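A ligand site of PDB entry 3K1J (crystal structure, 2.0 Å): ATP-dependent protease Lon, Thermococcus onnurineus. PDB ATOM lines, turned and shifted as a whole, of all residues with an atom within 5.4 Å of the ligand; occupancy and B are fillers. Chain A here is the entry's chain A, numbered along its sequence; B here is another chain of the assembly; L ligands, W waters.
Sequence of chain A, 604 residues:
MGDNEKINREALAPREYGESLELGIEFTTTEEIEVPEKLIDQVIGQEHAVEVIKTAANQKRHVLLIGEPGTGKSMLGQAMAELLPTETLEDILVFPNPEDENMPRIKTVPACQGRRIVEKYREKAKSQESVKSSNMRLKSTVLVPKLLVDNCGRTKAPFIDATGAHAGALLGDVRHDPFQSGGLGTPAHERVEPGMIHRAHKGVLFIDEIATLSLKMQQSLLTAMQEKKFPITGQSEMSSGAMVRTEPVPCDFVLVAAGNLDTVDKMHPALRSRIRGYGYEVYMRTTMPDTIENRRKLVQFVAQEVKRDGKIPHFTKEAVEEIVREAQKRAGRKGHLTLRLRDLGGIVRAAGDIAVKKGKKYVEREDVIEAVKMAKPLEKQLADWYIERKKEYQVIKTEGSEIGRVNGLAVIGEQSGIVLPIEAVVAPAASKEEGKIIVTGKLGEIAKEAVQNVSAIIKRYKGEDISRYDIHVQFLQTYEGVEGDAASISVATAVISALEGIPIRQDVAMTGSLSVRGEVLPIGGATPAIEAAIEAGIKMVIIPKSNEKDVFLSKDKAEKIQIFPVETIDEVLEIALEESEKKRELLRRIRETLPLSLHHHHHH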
ATOM      1  N   GLN A  42     -17.236 -23.174 -11.764  1.00  0.00           N
ATOM      2  CA  GLN A  42     -17.977 -22.831 -12.976  1.00  0.00           C
ATOM      3  C   GLN A  42     -18.934 -21.666 -12.739  1.00  0.00           C
ATOM      4  O   GLN A  42     -19.402 -21.042 -13.690  1.00  0.00           O
ATOM      5  CB  GLN A  42     -18.748 -24.056 -13.462  1.00  0.00           C
ATOM      6  CG  GLN A  42     -17.857 -25.109 -14.104  1.00  0.00           C
ATOM      7  CD  GLN A  42     -18.645 -26.241 -14.695  1.00  0.00           C
ATOM      8  OE1 GLN A  42     -19.713 -26.040 -15.266  1.00  0.00           O
ATOM      9  NE2 GLN A  42     -18.109 -27.447 -14.582  1.00  0.00           N
ATOM     10  N   VAL A  43     -19.229 -21.373 -11.468  1.00  0.00           N
ATOM     11  CA  VAL A  43     -20.112 -20.270 -11.123  1.00  0.00           C
ATOM     12  C   VAL A  43     -19.417 -18.959 -11.479  1.00  0.00           C
ATOM     13  O   VAL A  43     -18.298 -18.682 -11.022  1.00  0.00           O
ATOM     14  CB  VAL A  43     -20.458 -20.269  -9.605  1.00  0.00           C
ATOM     15  CG1 VAL A  43     -21.296 -19.043  -9.254  1.00  0.00           C
ATOM     16  CG2 VAL A  43     -21.210 -21.542  -9.263  1.00  0.00           C
ATOM     17  N   ILE A  44     -20.084 -18.160 -12.291  1.00  0.00           N
ATOM     18  CA  ILE A  44     -19.557 -16.893 -12.778  1.00  0.00           C
ATOM     19  C   ILE A  44     -20.210 -15.676 -12.134  1.00  0.00           C
ATOM     20  O   ILE A  44     -21.421 -15.643 -11.920  1.00  0.00           O
ATOM     21  CB  ILE A  44     -19.743 -16.849 -14.322  1.00  0.00           C
ATOM     22  CG1 ILE A  44     -18.936 -17.984 -14.960  1.00  0.00           C
ATOM     23  CG2 ILE A  44     -19.335 -15.507 -14.894  1.00  0.00           C
ATOM     24  CD1 ILE A  44     -19.435 -18.404 -16.304  1.00  0.00           C
ATOM     25  N   GLY A  45     -19.377 -14.692 -11.807  1.00  0.00           N
ATOM     26  CA  GLY A  45     -19.844 -13.437 -11.240  1.00  0.00           C
ATOM     27  C   GLY A  45     -20.462 -13.298  -9.854  1.00  0.00           C
ATOM     28  O   GLY A  45     -20.804 -12.172  -9.451  1.00  0.00           O
ATOM     29  N   GLN A  46     -20.613 -14.385  -9.105  1.00  0.00           N
ATOM     30  CA  GLN A  46     -21.238 -14.276  -7.772  1.00  0.00           C
ATOM     31  C   GLN A  46     -20.173 -14.533  -6.714  1.00  0.00           C
ATOM     32  O   GLN A  46     -20.371 -15.372  -5.818  1.00  0.00           O
ATOM     33  CB  GLN A  46     -22.357 -15.299  -7.622  1.00  0.00           C
ATOM     34  CG  GLN A  46     -23.478 -15.201  -8.659  1.00  0.00           C
ATOM     35  CD  GLN A  46     -24.448 -14.067  -8.367  1.00  0.00           C
ATOM     36  OE1 GLN A  46     -24.366 -13.407  -7.329  1.00  0.00           O
ATOM     37  NE2 GLN A  46     -25.379 -13.846  -9.293  1.00  0.00           N
ATOM     38  N   GLU A  68     -33.385 -13.522  -8.321  1.00  0.00           N
ATOM     39  CA  GLU A  68     -34.277 -13.766  -9.465  1.00  0.00           C
ATOM     40  C   GLU A  68     -34.088 -15.191  -9.951  1.00  0.00           C
ATOM     41  O   GLU A  68     -33.053 -15.786  -9.721  1.00  0.00           O
ATOM     42  CB  GLU A  68     -33.928 -12.831 -10.625  1.00  0.00           C
ATOM     43  CG  GLU A  68     -34.153 -11.357 -10.376  1.00  0.00           C
ATOM     44  CD  GLU A  68     -33.843 -10.515 -11.605  1.00  0.00           C
ATOM     45  OE1 GLU A  68     -33.662 -11.094 -12.710  1.00  0.00           O
ATOM     46  OE2 GLU A  68     -33.790  -9.275 -11.482  1.00  0.00           O
ATOM     47  N   PRO A  69     -35.100 -15.751 -10.635  1.00  0.00           N
ATOM     48  CA  PRO A  69     -34.906 -17.132 -11.107  1.00  0.00           C
ATOM     49  C   PRO A  69     -33.821 -17.197 -12.193  1.00  0.00           C
ATOM     50  O   PRO A  69     -33.613 -16.216 -12.916  1.00  0.00           O
ATOM     51  CB  PRO A  69     -36.285 -17.514 -11.638  1.00  0.00           C
ATOM     52  CG  PRO A  69     -36.862 -16.202 -12.072  1.00  0.00           C
ATOM     53  CD  PRO A  69     -36.448 -15.254 -10.961  1.00  0.00           C
ATOM     54  N   GLY A  70     -33.133 -18.335 -12.274  1.00  0.00           N
ATOM     55  CA  GLY A  70     -32.099 -18.507 -13.276  1.00  0.00           C
ATOM     56  C   GLY A  70     -30.862 -17.667 -13.024  1.00  0.00           C
ATOM     57  O   GLY A  70     -30.224 -17.166 -13.948  1.00  0.00           O
ATOM     58  N   THR A  71     -30.510 -17.545 -11.755  1.00  0.00           N
ATOM     59  CA  THR A  71     -29.366 -16.752 -11.370  1.00  0.00           C
ATOM     60  C   THR A  71     -28.295 -17.615 -10.697  1.00  0.00           C
ATOM     61  O   THR A  71     -27.305 -17.103 -10.167  1.00  0.00           O
ATOM     62  CB  THR A  71     -29.837 -15.590 -10.461  1.00  0.00           C
ATOM     63  OG1 THR A  71     -28.804 -14.606 -10.370  1.00  0.00           O
ATOM     64  CG2 THR A  71     -30.223 -16.083  -9.094  1.00  0.00           C
ATOM     65  N   GLY A  72     -28.516 -18.919 -10.715  1.00  0.00           N
ATOM     66  CA  GLY A  72     -27.562 -19.865 -10.166  1.00  0.00           C
ATOM     67  C   GLY A  72     -27.743 -20.326  -8.734  1.00  0.00           C
ATOM     68  O   GLY A  72     -26.793 -20.836  -8.132  1.00  0.00           O
ATOM     69  N   LYS A  73     -28.945 -20.169  -8.164  1.00  0.00           N
ATOM     70  CA  LYS A  73     -29.149 -20.598  -6.784  1.00  0.00           C
ATOM     71  C   LYS A  73     -29.021 -22.106  -6.642  1.00  0.00           C
ATOM     72  O   LYS A  73     -28.289 -22.592  -5.782  1.00  0.00           O
ATOM     73  CB  LYS A  73     -30.527 -20.110  -6.287  1.00  0.00           C
ATOM     74  CG  LYS A  73     -30.647 -18.584  -6.324  1.00  0.00           C
ATOM     75  CD  LYS A  73     -31.954 -18.047  -5.725  1.00  0.00           C
ATOM     76  CE  LYS A  73     -33.196 -18.557  -6.469  1.00  0.00           C
ATOM     77  NZ  LYS A  73     -33.229 -18.127  -7.894  1.00  0.00           N
ATOM     78  N   SER A  74     -29.716 -22.866  -7.489  1.00  0.00           N
ATOM     79  CA  SER A  74     -29.628 -24.329  -7.439  1.00  0.00           C
ATOM     80  C   SER A  74     -28.197 -24.801  -7.786  1.00  0.00           C
ATOM     81  O   SER A  74     -27.675 -25.753  -7.205  1.00  0.00           O
ATOM     82  CB  SER A  74     -30.601 -24.932  -8.429  1.00  0.00           C
ATOM     83  OG  SER A  74     -30.472 -26.343  -8.433  1.00  0.00           O
ATOM     84  N   MET A  75     -27.587 -24.136  -8.757  1.00  0.00           N
ATOM     85  CA  MET A  75     -26.223 -24.477  -9.166  1.00  0.00           C
ATOM     86  C   MET A  75     -25.301 -24.361  -7.945  1.00  0.00           C
ATOM     87  O   MET A  75     -24.461 -25.220  -7.708  1.00  0.00           O
ATOM     88  CB  MET A  75     -25.751 -23.534 -10.282  1.00  0.00           C
ATOM     89  CG  MET A  75     -24.474 -24.000 -10.998  1.00  0.00           C
ATOM     90  SD  MET A  75     -23.846 -22.731 -12.116  1.00  0.00           S
ATOM     91  CE  MET A  75     -22.162 -23.433 -12.507  1.00  0.00           C
ATOM     92  N   LEU A  76     -25.484 -23.300  -7.156  1.00  0.00           N
ATOM     93  CA  LEU A  76     -24.669 -23.117  -5.954  1.00  0.00           C
ATOM     94  C   LEU A  76     -24.910 -24.229  -4.937  1.00  0.00           C
ATOM     95  O   LEU A  76     -23.981 -24.710  -4.284  1.00  0.00           O
ATOM     96  CB  LEU A  76     -24.968 -21.748  -5.320  1.00  0.00           C
ATOM     97  CG  LEU A  76     -24.360 -20.552  -6.036  1.00  0.00           C
ATOM     98  CD1 LEU A  76     -24.965 -19.253  -5.509  1.00  0.00           C
ATOM     99  CD2 LEU A  76     -22.837 -20.563  -5.845  1.00  0.00           C
ATOM    100  N   PHE A 206     -31.778 -28.901  -0.926  1.00  0.00           N
ATOM    101  CA  PHE A 206     -32.058 -27.644  -1.623  1.00  0.00           C
ATOM    102  C   PHE A 206     -33.558 -27.410  -1.706  1.00  0.00           C
ATOM    103  O   PHE A 206     -34.305 -28.304  -2.102  1.00  0.00           O
ATOM    104  CB  PHE A 206     -31.487 -27.669  -3.057  1.00  0.00           C
ATOM    105  CG  PHE A 206     -31.742 -26.396  -3.841  1.00  0.00           C
ATOM    106  CD1 PHE A 206     -31.044 -25.227  -3.557  1.00  0.00           C
ATOM    107  CD2 PHE A 206     -32.708 -26.363  -4.847  1.00  0.00           C
ATOM    108  CE1 PHE A 206     -31.302 -24.039  -4.247  1.00  0.00           C
ATOM    109  CE2 PHE A 206     -32.986 -25.187  -5.544  1.00  0.00           C
ATOM    110  CZ  PHE A 206     -32.282 -24.016  -5.253  1.00  0.00           C
ATOM    111  N   ASP A 208     -36.019 -24.384  -3.160  1.00  0.00           N
ATOM    112  CA  ASP A 208     -36.302 -23.075  -3.736  1.00  0.00           C
ATOM    113  C   ASP A 208     -37.762 -22.768  -3.349  1.00  0.00           C
ATOM    114  O   ASP A 208     -38.520 -23.699  -3.024  1.00  0.00           O
ATOM    115  CB  ASP A 208     -36.111 -23.126  -5.251  1.00  0.00           C
ATOM    116  CG  ASP A 208     -36.087 -21.747  -5.902  1.00  0.00           C
ATOM    117  OD1 ASP A 208     -36.138 -20.718  -5.184  1.00  0.00           O
ATOM    118  OD2 ASP A 208     -36.012 -21.690  -7.139  1.00  0.00           O
ATOM    119  N   PHE A 301     -18.015 -19.804 -19.805  1.00  0.00           N
ATOM    120  CA  PHE A 301     -19.455 -20.083 -19.689  1.00  0.00           C
ATOM    121  C   PHE A 301     -20.004 -20.856 -20.906  1.00  0.00           C
ATOM    122  O   PHE A 301     -20.637 -21.909 -20.760  1.00  0.00           O
ATOM    123  CB  PHE A 301     -20.226 -18.762 -19.549  1.00  0.00           C
ATOM    124  CG  PHE A 301     -21.717 -18.941 -19.500  1.00  0.00           C
ATOM    125  CD1 PHE A 301     -22.334 -19.500 -18.390  1.00  0.00           C
ATOM    126  CD2 PHE A 301     -22.503 -18.577 -20.592  1.00  0.00           C
ATOM    127  CE1 PHE A 301     -23.707 -19.714 -18.363  1.00  0.00           C
ATOM    128  CE2 PHE A 301     -23.889 -18.783 -20.583  1.00  0.00           C
ATOM    129  CZ  PHE A 301     -24.499 -19.351 -19.462  1.00  0.00           C
ATOM    130  N   GLN A 304     -18.574 -24.434 -20.957  1.00  0.00           N
ATOM    131  CA  GLN A 304     -19.135 -25.361 -19.978  1.00  0.00           C
ATOM    132  C   GLN A 304     -20.576 -25.697 -20.300  1.00  0.00           C
ATOM    133  O   GLN A 304     -21.029 -26.802 -19.992  1.00  0.00           O
ATOM    134  CB  GLN A 304     -18.999 -24.806 -18.552  1.00  0.00           C
ATOM    135  CG  GLN A 304     -19.593 -23.425 -18.305  1.00  0.00           C
ATOM    136  CD  GLN A 304     -19.124 -22.816 -16.984  1.00  0.00           C
ATOM    137  OE1 GLN A 304     -17.947 -22.913 -16.634  1.00  0.00           O
ATOM    138  NE2 GLN A 304     -20.028 -22.177 -16.271  1.00  0.00           N
ATOM    139  N   GLU A 305     -21.291 -24.764 -20.932  1.00  0.00           N
ATOM    140  CA  GLU A 305     -22.687 -24.995 -21.296  1.00  0.00           C
ATOM    141  C   GLU A 305     -22.754 -25.998 -22.439  1.00  0.00           C
ATOM    142  O   GLU A 305     -23.586 -26.906 -22.446  1.00  0.00           O
ATOM    143  CB  GLU A 305     -23.351 -23.682 -21.727  1.00  0.00           C
ATOM    144  CG  GLU A 305     -23.616 -22.704 -20.601  1.00  0.00           C
ATOM    145  CD  GLU A 305     -24.592 -23.260 -19.580  1.00  0.00           C
ATOM    146  OE1 GLU A 305     -25.638 -23.813 -19.995  1.00  0.00           O
ATOM    147  OE2 GLU A 305     -24.326 -23.136 -18.359  1.00  0.00           O
ATOM    148  N   ARG A 308     -21.801 -29.327 -20.888  1.00  0.00           N
ATOM    149  CA  ARG A 308     -22.853 -29.865 -20.054  1.00  0.00           C
ATOM    150  C   ARG A 308     -24.034 -30.321 -20.894  1.00  0.00           C
ATOM    151  O   ARG A 308     -24.669 -31.323 -20.577  1.00  0.00           O
ATOM    152  CB  ARG A 308     -23.308 -28.822 -19.021  1.00  0.00           C
ATOM    153  CG  ARG A 308     -23.972 -29.433 -17.799  1.00  0.00           C
ATOM    154  CD  ARG A 308     -24.416 -28.357 -16.807  1.00  0.00           C
ATOM    155  NE  ARG A 308     -23.394 -27.319 -16.640  1.00  0.00           N
ATOM    156  CZ  ARG A 308     -23.463 -26.325 -15.773  1.00  0.00           C
ATOM    157  NH1 ARG A 308     -24.521 -26.209 -14.975  1.00  0.00           N
ATOM    158  NH2 ARG A 308     -22.482 -25.416 -15.704  1.00  0.00           N
ATOM    159  N   LEU A 339     -25.991 -11.367 -15.355  1.00  0.00           N
ATOM    160  CA  LEU A 339     -25.678 -12.591 -14.638  1.00  0.00           C
ATOM    161  C   LEU A 339     -26.928 -13.474 -14.667  1.00  0.00           C
ATOM    162  O   LEU A 339     -27.071 -14.425 -13.897  1.00  0.00           O
ATOM    163  CB  LEU A 339     -25.216 -12.307 -13.202  1.00  0.00           C
ATOM    164  CG  LEU A 339     -23.746 -11.864 -13.076  1.00  0.00           C
ATOM    165  CD1 LEU A 339     -23.361 -11.788 -11.606  1.00  0.00           C
ATOM    166  CD2 LEU A 339     -22.819 -12.850 -13.797  1.00  0.00           C
ATOM    167  N   LEU A 341     -27.769 -15.893 -16.234  1.00  0.00           N
ATOM    168  CA  LEU A 341     -27.149 -16.918 -17.053  1.00  0.00           C
ATOM    169  C   LEU A 341     -27.987 -18.110 -17.467  1.00  0.00           C
ATOM    170  O   LEU A 341     -27.598 -18.846 -18.373  1.00  0.00           O
ATOM    171  CB  LEU A 341     -25.816 -17.326 -16.397  1.00  0.00           C
ATOM    172  CG  LEU A 341     -24.937 -16.063 -16.273  1.00  0.00           C
ATOM    173  CD1 LEU A 341     -23.557 -16.369 -15.672  1.00  0.00           C
ATOM    174  CD2 LEU A 341     -24.774 -15.451 -17.654  1.00  0.00           C
ATOM    175  N   ARG A 342     -29.139 -18.306 -16.822  1.00  0.00           N
ATOM    176  CA  ARG A 342     -30.014 -19.387 -17.238  1.00  0.00           C
ATOM    177  C   ARG A 342     -30.545 -18.951 -18.620  1.00  0.00           C
ATOM    178  O   ARG A 342     -30.587 -19.753 -19.549  1.00  0.00           O
ATOM    179  CB  ARG A 342     -31.191 -19.578 -16.278  1.00  0.00           C
ATOM    180  CG  ARG A 342     -32.056 -20.792 -16.641  1.00  0.00           C
ATOM    181  CD  ARG A 342     -33.252 -20.948 -15.711  1.00  0.00           C
ATOM    182  NE  ARG A 342     -34.230 -19.881 -15.916  1.00  0.00           N
ATOM    183  CZ  ARG A 342     -35.330 -19.735 -15.179  1.00  0.00           C
ATOM    184  NH1 ARG A 342     -35.588 -20.589 -14.195  1.00  0.00           N
ATOM    185  NH2 ARG A 342     -36.179 -18.747 -15.432  1.00  0.00           N
ATOM    186  N   ARG A 349     -27.885 -22.815 -25.959  1.00  0.00           N
ATOM    187  CA  ARG A 349     -28.459 -24.075 -26.413  1.00  0.00           C
ATOM    188  C   ARG A 349     -29.289 -23.923 -27.676  1.00  0.00           C
ATOM    189  O   ARG A 349     -29.250 -24.798 -28.553  1.00  0.00           O
ATOM    190  CB  ARG A 349     -29.265 -24.765 -25.297  1.00  0.00           C
ATOM    191  CG  ARG A 349     -28.367 -25.382 -24.198  1.00  0.00           C
ATOM    192  CD  ARG A 349     -29.160 -26.198 -23.159  1.00  0.00           C
ATOM    193  NE  ARG A 349     -30.106 -25.354 -22.437  1.00  0.00           N
ATOM    194  CZ  ARG A 349     -29.759 -24.488 -21.502  1.00  0.00           C
ATOM    195  NH1 ARG A 349     -28.488 -24.351 -21.152  1.00  0.00           N
ATOM    196  NH2 ARG A 349     -30.685 -23.740 -20.920  1.00  0.00           N
ATOM    197  N   SER B 273     -39.453 -24.325 -13.650  1.00  0.00           N
ATOM    198  CA  SER B 273     -38.073 -23.914 -13.884  1.00  0.00           C
ATOM    199  C   SER B 273     -37.413 -24.778 -14.943  1.00  0.00           C
ATOM    200  O   SER B 273     -36.677 -24.286 -15.802  1.00  0.00           O
ATOM    201  CB  SER B 273     -37.263 -23.970 -12.597  1.00  0.00           C
ATOM    202  OG  SER B 273     -37.759 -23.018 -11.670  1.00  0.00           O
ATOM    203  N   TYR B 278     -34.833 -25.021 -19.690  1.00  0.00           N
ATOM    204  CA  TYR B 278     -34.208 -25.856 -20.701  1.00  0.00           C
ATOM    205  C   TYR B 278     -35.004 -26.232 -21.961  1.00  0.00           C
ATOM    206  O   TYR B 278     -34.516 -26.987 -22.801  1.00  0.00           O
ATOM    207  CB  TYR B 278     -33.655 -27.107 -20.028  1.00  0.00           C
ATOM    208  CG  TYR B 278     -32.675 -26.777 -18.917  1.00  0.00           C
ATOM    209  CD1 TYR B 278     -33.126 -26.269 -17.689  1.00  0.00           C
ATOM    210  CD2 TYR B 278     -31.294 -26.897 -19.108  1.00  0.00           C
ATOM    211  CE1 TYR B 278     -32.229 -25.905 -16.674  1.00  0.00           C
ATOM    212  CE2 TYR B 278     -30.386 -26.536 -18.113  1.00  0.00           C
ATOM    213  CZ  TYR B 278     -30.864 -26.041 -16.901  1.00  0.00           C
ATOM    214  OH  TYR B 278     -29.970 -25.701 -15.905  1.00  0.00           O
HETATM  215  P1  LIG L   1     -31.987 -20.716 -10.068  1.00  0.00           P
HETATM  216  O1  LIG L   1     -31.550 -19.456  -9.428  1.00  0.00           O
HETATM  217  O2  LIG L   1     -31.918 -21.891  -9.181  1.00  0.00           O
HETATM  218  O3  LIG L   1     -33.262 -20.592 -10.782  1.00  0.00           O
HETATM  219  P2  LIG L   1     -30.252 -22.365 -11.806  1.00  0.00           P
HETATM  220  O4  LIG L   1     -29.260 -22.797 -10.814  1.00  0.00           O
HETATM  221  O5  LIG L   1     -31.281 -23.326 -12.111  1.00  0.00           O
HETATM  222  O6  LIG L   1     -31.001 -21.026 -11.276  1.00  0.00           O
HETATM  223  O7  LIG L   1     -29.508 -21.981 -13.166  1.00  0.00           O
HETATM  224  C1  LIG L   1     -29.707 -22.460 -14.505  1.00  0.00           C
HETATM  225  C2  LIG L   1     -28.479 -22.712 -15.272  1.00  0.00           C
HETATM  226  O8  LIG L   1     -27.960 -21.385 -15.415  1.00  0.00           O
HETATM  227  C3  LIG L   1     -27.318 -23.365 -14.501  1.00  0.00           C
HETATM  228  O9  LIG L   1     -27.559 -24.739 -14.285  1.00  0.00           O
HETATM  229  C4  LIG L   1     -26.122 -22.925 -15.379  1.00  0.00           C
HETATM  230  O10 LIG L   1     -26.197 -23.545 -16.597  1.00  0.00           O
HETATM  231  C5  LIG L   1     -26.453 -21.451 -15.535  1.00  0.00           C
HETATM  232  N1  LIG L   1     -26.338 -20.299 -14.520  1.00  0.00           N
HETATM  233  C6  LIG L   1     -27.089 -19.457 -13.758  1.00  0.00           C
HETATM  234  N2  LIG L   1     -26.365 -18.620 -13.051  1.00  0.00           N
HETATM  235  C7  LIG L   1     -25.037 -18.931 -13.346  1.00  0.00           C
HETATM  236  C8  LIG L   1     -23.736 -18.393 -12.910  1.00  0.00           C
HETATM  237  N3  LIG L   1     -23.592 -17.359 -12.052  1.00  0.00           N
HETATM  238  N4  LIG L   1     -22.594 -18.988 -13.433  1.00  0.00           N
HETATM  239  C9  LIG L   1     -22.723 -19.995 -14.309  1.00  0.00           C
HETATM  240  N5  LIG L   1     -23.884 -20.557 -14.773  1.00  0.00           N
HETATM  241  C10 LIG L   1     -25.012 -19.972 -14.247  1.00  0.00           C
HETATM  242  O   HOH W   1     -22.747 -22.544 -16.457  1.00  0.00           O
HETATM  243  O   HOH W   2     -28.129 -22.360 -18.834  1.00  0.00           O
HETATM  244  O   HOH W   3     -35.355 -19.677  -8.759  1.00  0.00           O
HETATM  245  O   HOH W   4     -28.343 -25.561 -11.891  1.00  0.00           O
HETATM  246  O   HOH W   5     -34.076 -23.225  -8.350  1.00  0.00           O
HETATM  247  O   HOH W   6     -25.932 -15.591 -11.708  1.00  0.00           O
HETATM  248  O   HOH W   7     -33.766 -22.346 -13.247  1.00  0.00           O
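N of Ile 44 sits at hydrogen-bond distance from N4 of the ligand (2.9 Å). The guanidinium group (NH1) of Arg 308 is in hydrogen-bond range of an oxygen (O9) of the ligand. O1 of the ligand is in salt-bridge range of NZ of Lys 73. N of Gly 72 is in hydrogen-bond range of N2 of the ligand, at 3.2 Å. O9 of the ligand lies within hydrogen-bond range of OH of Tyr 278 of chain B (3.1 Å). The backbone NH (N) of Ser 74 sits at hydrogen-bond distance from an oxygen (O2) of the ligand, 2.9 Å away. N of Thr 71 lies within hydrogen-bond range of O1 of the ligand (3.2 Å). The backbone NH (N) of Gly 70 sits at hydrogen-bond distance from an oxygen (O3) of the ligand (2.7 Å). The side-chain carboxylate (OE2) of Glu 305 sits at hydrogen-bond distance from an oxygen (O10) of the ligand (2.6 Å). The backbone carbonyl oxygen of Ile 44 sits at hydrogen-bond distance from a nitrogen (N3) of the ligand. O4 of the ligand is in hydrogen-bond range of N of Met 75 (3.0 Å). An oxygen (O1) of the ligand is in hydrogen-bond range of the backbone NH (N) of Lys 73 (3.0 Å).
OE1 of Glu 305 lies within salt-bridge range of NH1 of Arg 349 (3.1 Å). OE2 of Glu 305 is in salt-bridge range of NH2 of Arg 308, at 3.96 Å. N of Arg 342 is in hydrogen-bond range of O of Gly 70 (3.3 Å). The side-chain amino group (NZ) of Lys 73 lies within hydrogen-bond range of the backbone carbonyl oxygen (O) of Glu 68, 3.0 Å away. The side-chain amide oxygen (OE1) of Gln 42 is in hydrogen-bond range of the guanidinium group (NH2) of Arg 308, 2.9 Å away. O of Gln 42 lies within hydrogen-bond range of NE2 of Gln 304, at 2.9 Å.
Merely in contact with the ligand: Arg 342 (3.4 Å), Leu 341 (3.4 Å), Gln 42 (3.5 Å), Val 43 (3.6 Å), Phe 301 (3.7 Å), Pro 69 (3.7 Å), Glu 68 (3.98 Å) and Gln 304 (3.98 Å). Hydrophobic or aromatic side chains that line the ligand: Val 43, Ile 44, Met 75, Phe 301 and Leu 341. 18 residues have an atom within 4 Å of the ligand: Gln 42, Val 43, Ile 44, Glu 68, Pro 69, Gly 70, Thr 71, Gly 72, Lys 73, Ser 74, Met 75, Phe 301, Gln 304, Glu 305, Arg 308, Leu 341, Arg 342 and Tyr 278 of chain B. Along chain A the residues within 4 Å of the ligand span positions 42 to 342. The nearest printed residue that does not touch the ligand is Gln 46 (4.02 Å).
Water W5 lies within hydrogen-bond range of O2 of the ligand (2.7 Å) and OD2 of Asp 208 (2.8 Å). Water W1 lies within hydrogen-bond range of OE2 of Glu 305 (2.5 Å), NE2 of Gln 304 (2.7 Å), N5 of the ligand (2.8 Å) and NH2 of Arg 308 (3.0 Å). Water W7 bridges the guanidinium group (NH1) of Arg 342 (2.7 Å) and an oxygen (O5) of the ligand (2.9 Å). Water W6 lies within hydrogen-bond range of the backbone carbonyl oxygen (O) of Thr 71 (2.6 Å), the backbone carbonyl oxygen (O) of Leu 339 (2.7 Å), a nitrogen (N3) of the ligand (3.0 Å) and the side-chain amide nitrogen (NE2) of Gln 46 (3.0 Å). Water W3 lies within hydrogen-bond range of OD2 of Asp 208, NZ of Lys 73 and O3 of the ligand. Water W2 lies within hydrogen-bond range of the guanidinium group (NH1) of Arg 349 (3.1 Å), the side-chain carboxylate (OE1) of Glu 305 (3.1 Å) and an oxygen (O10) of the ligand (3.2 Å).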
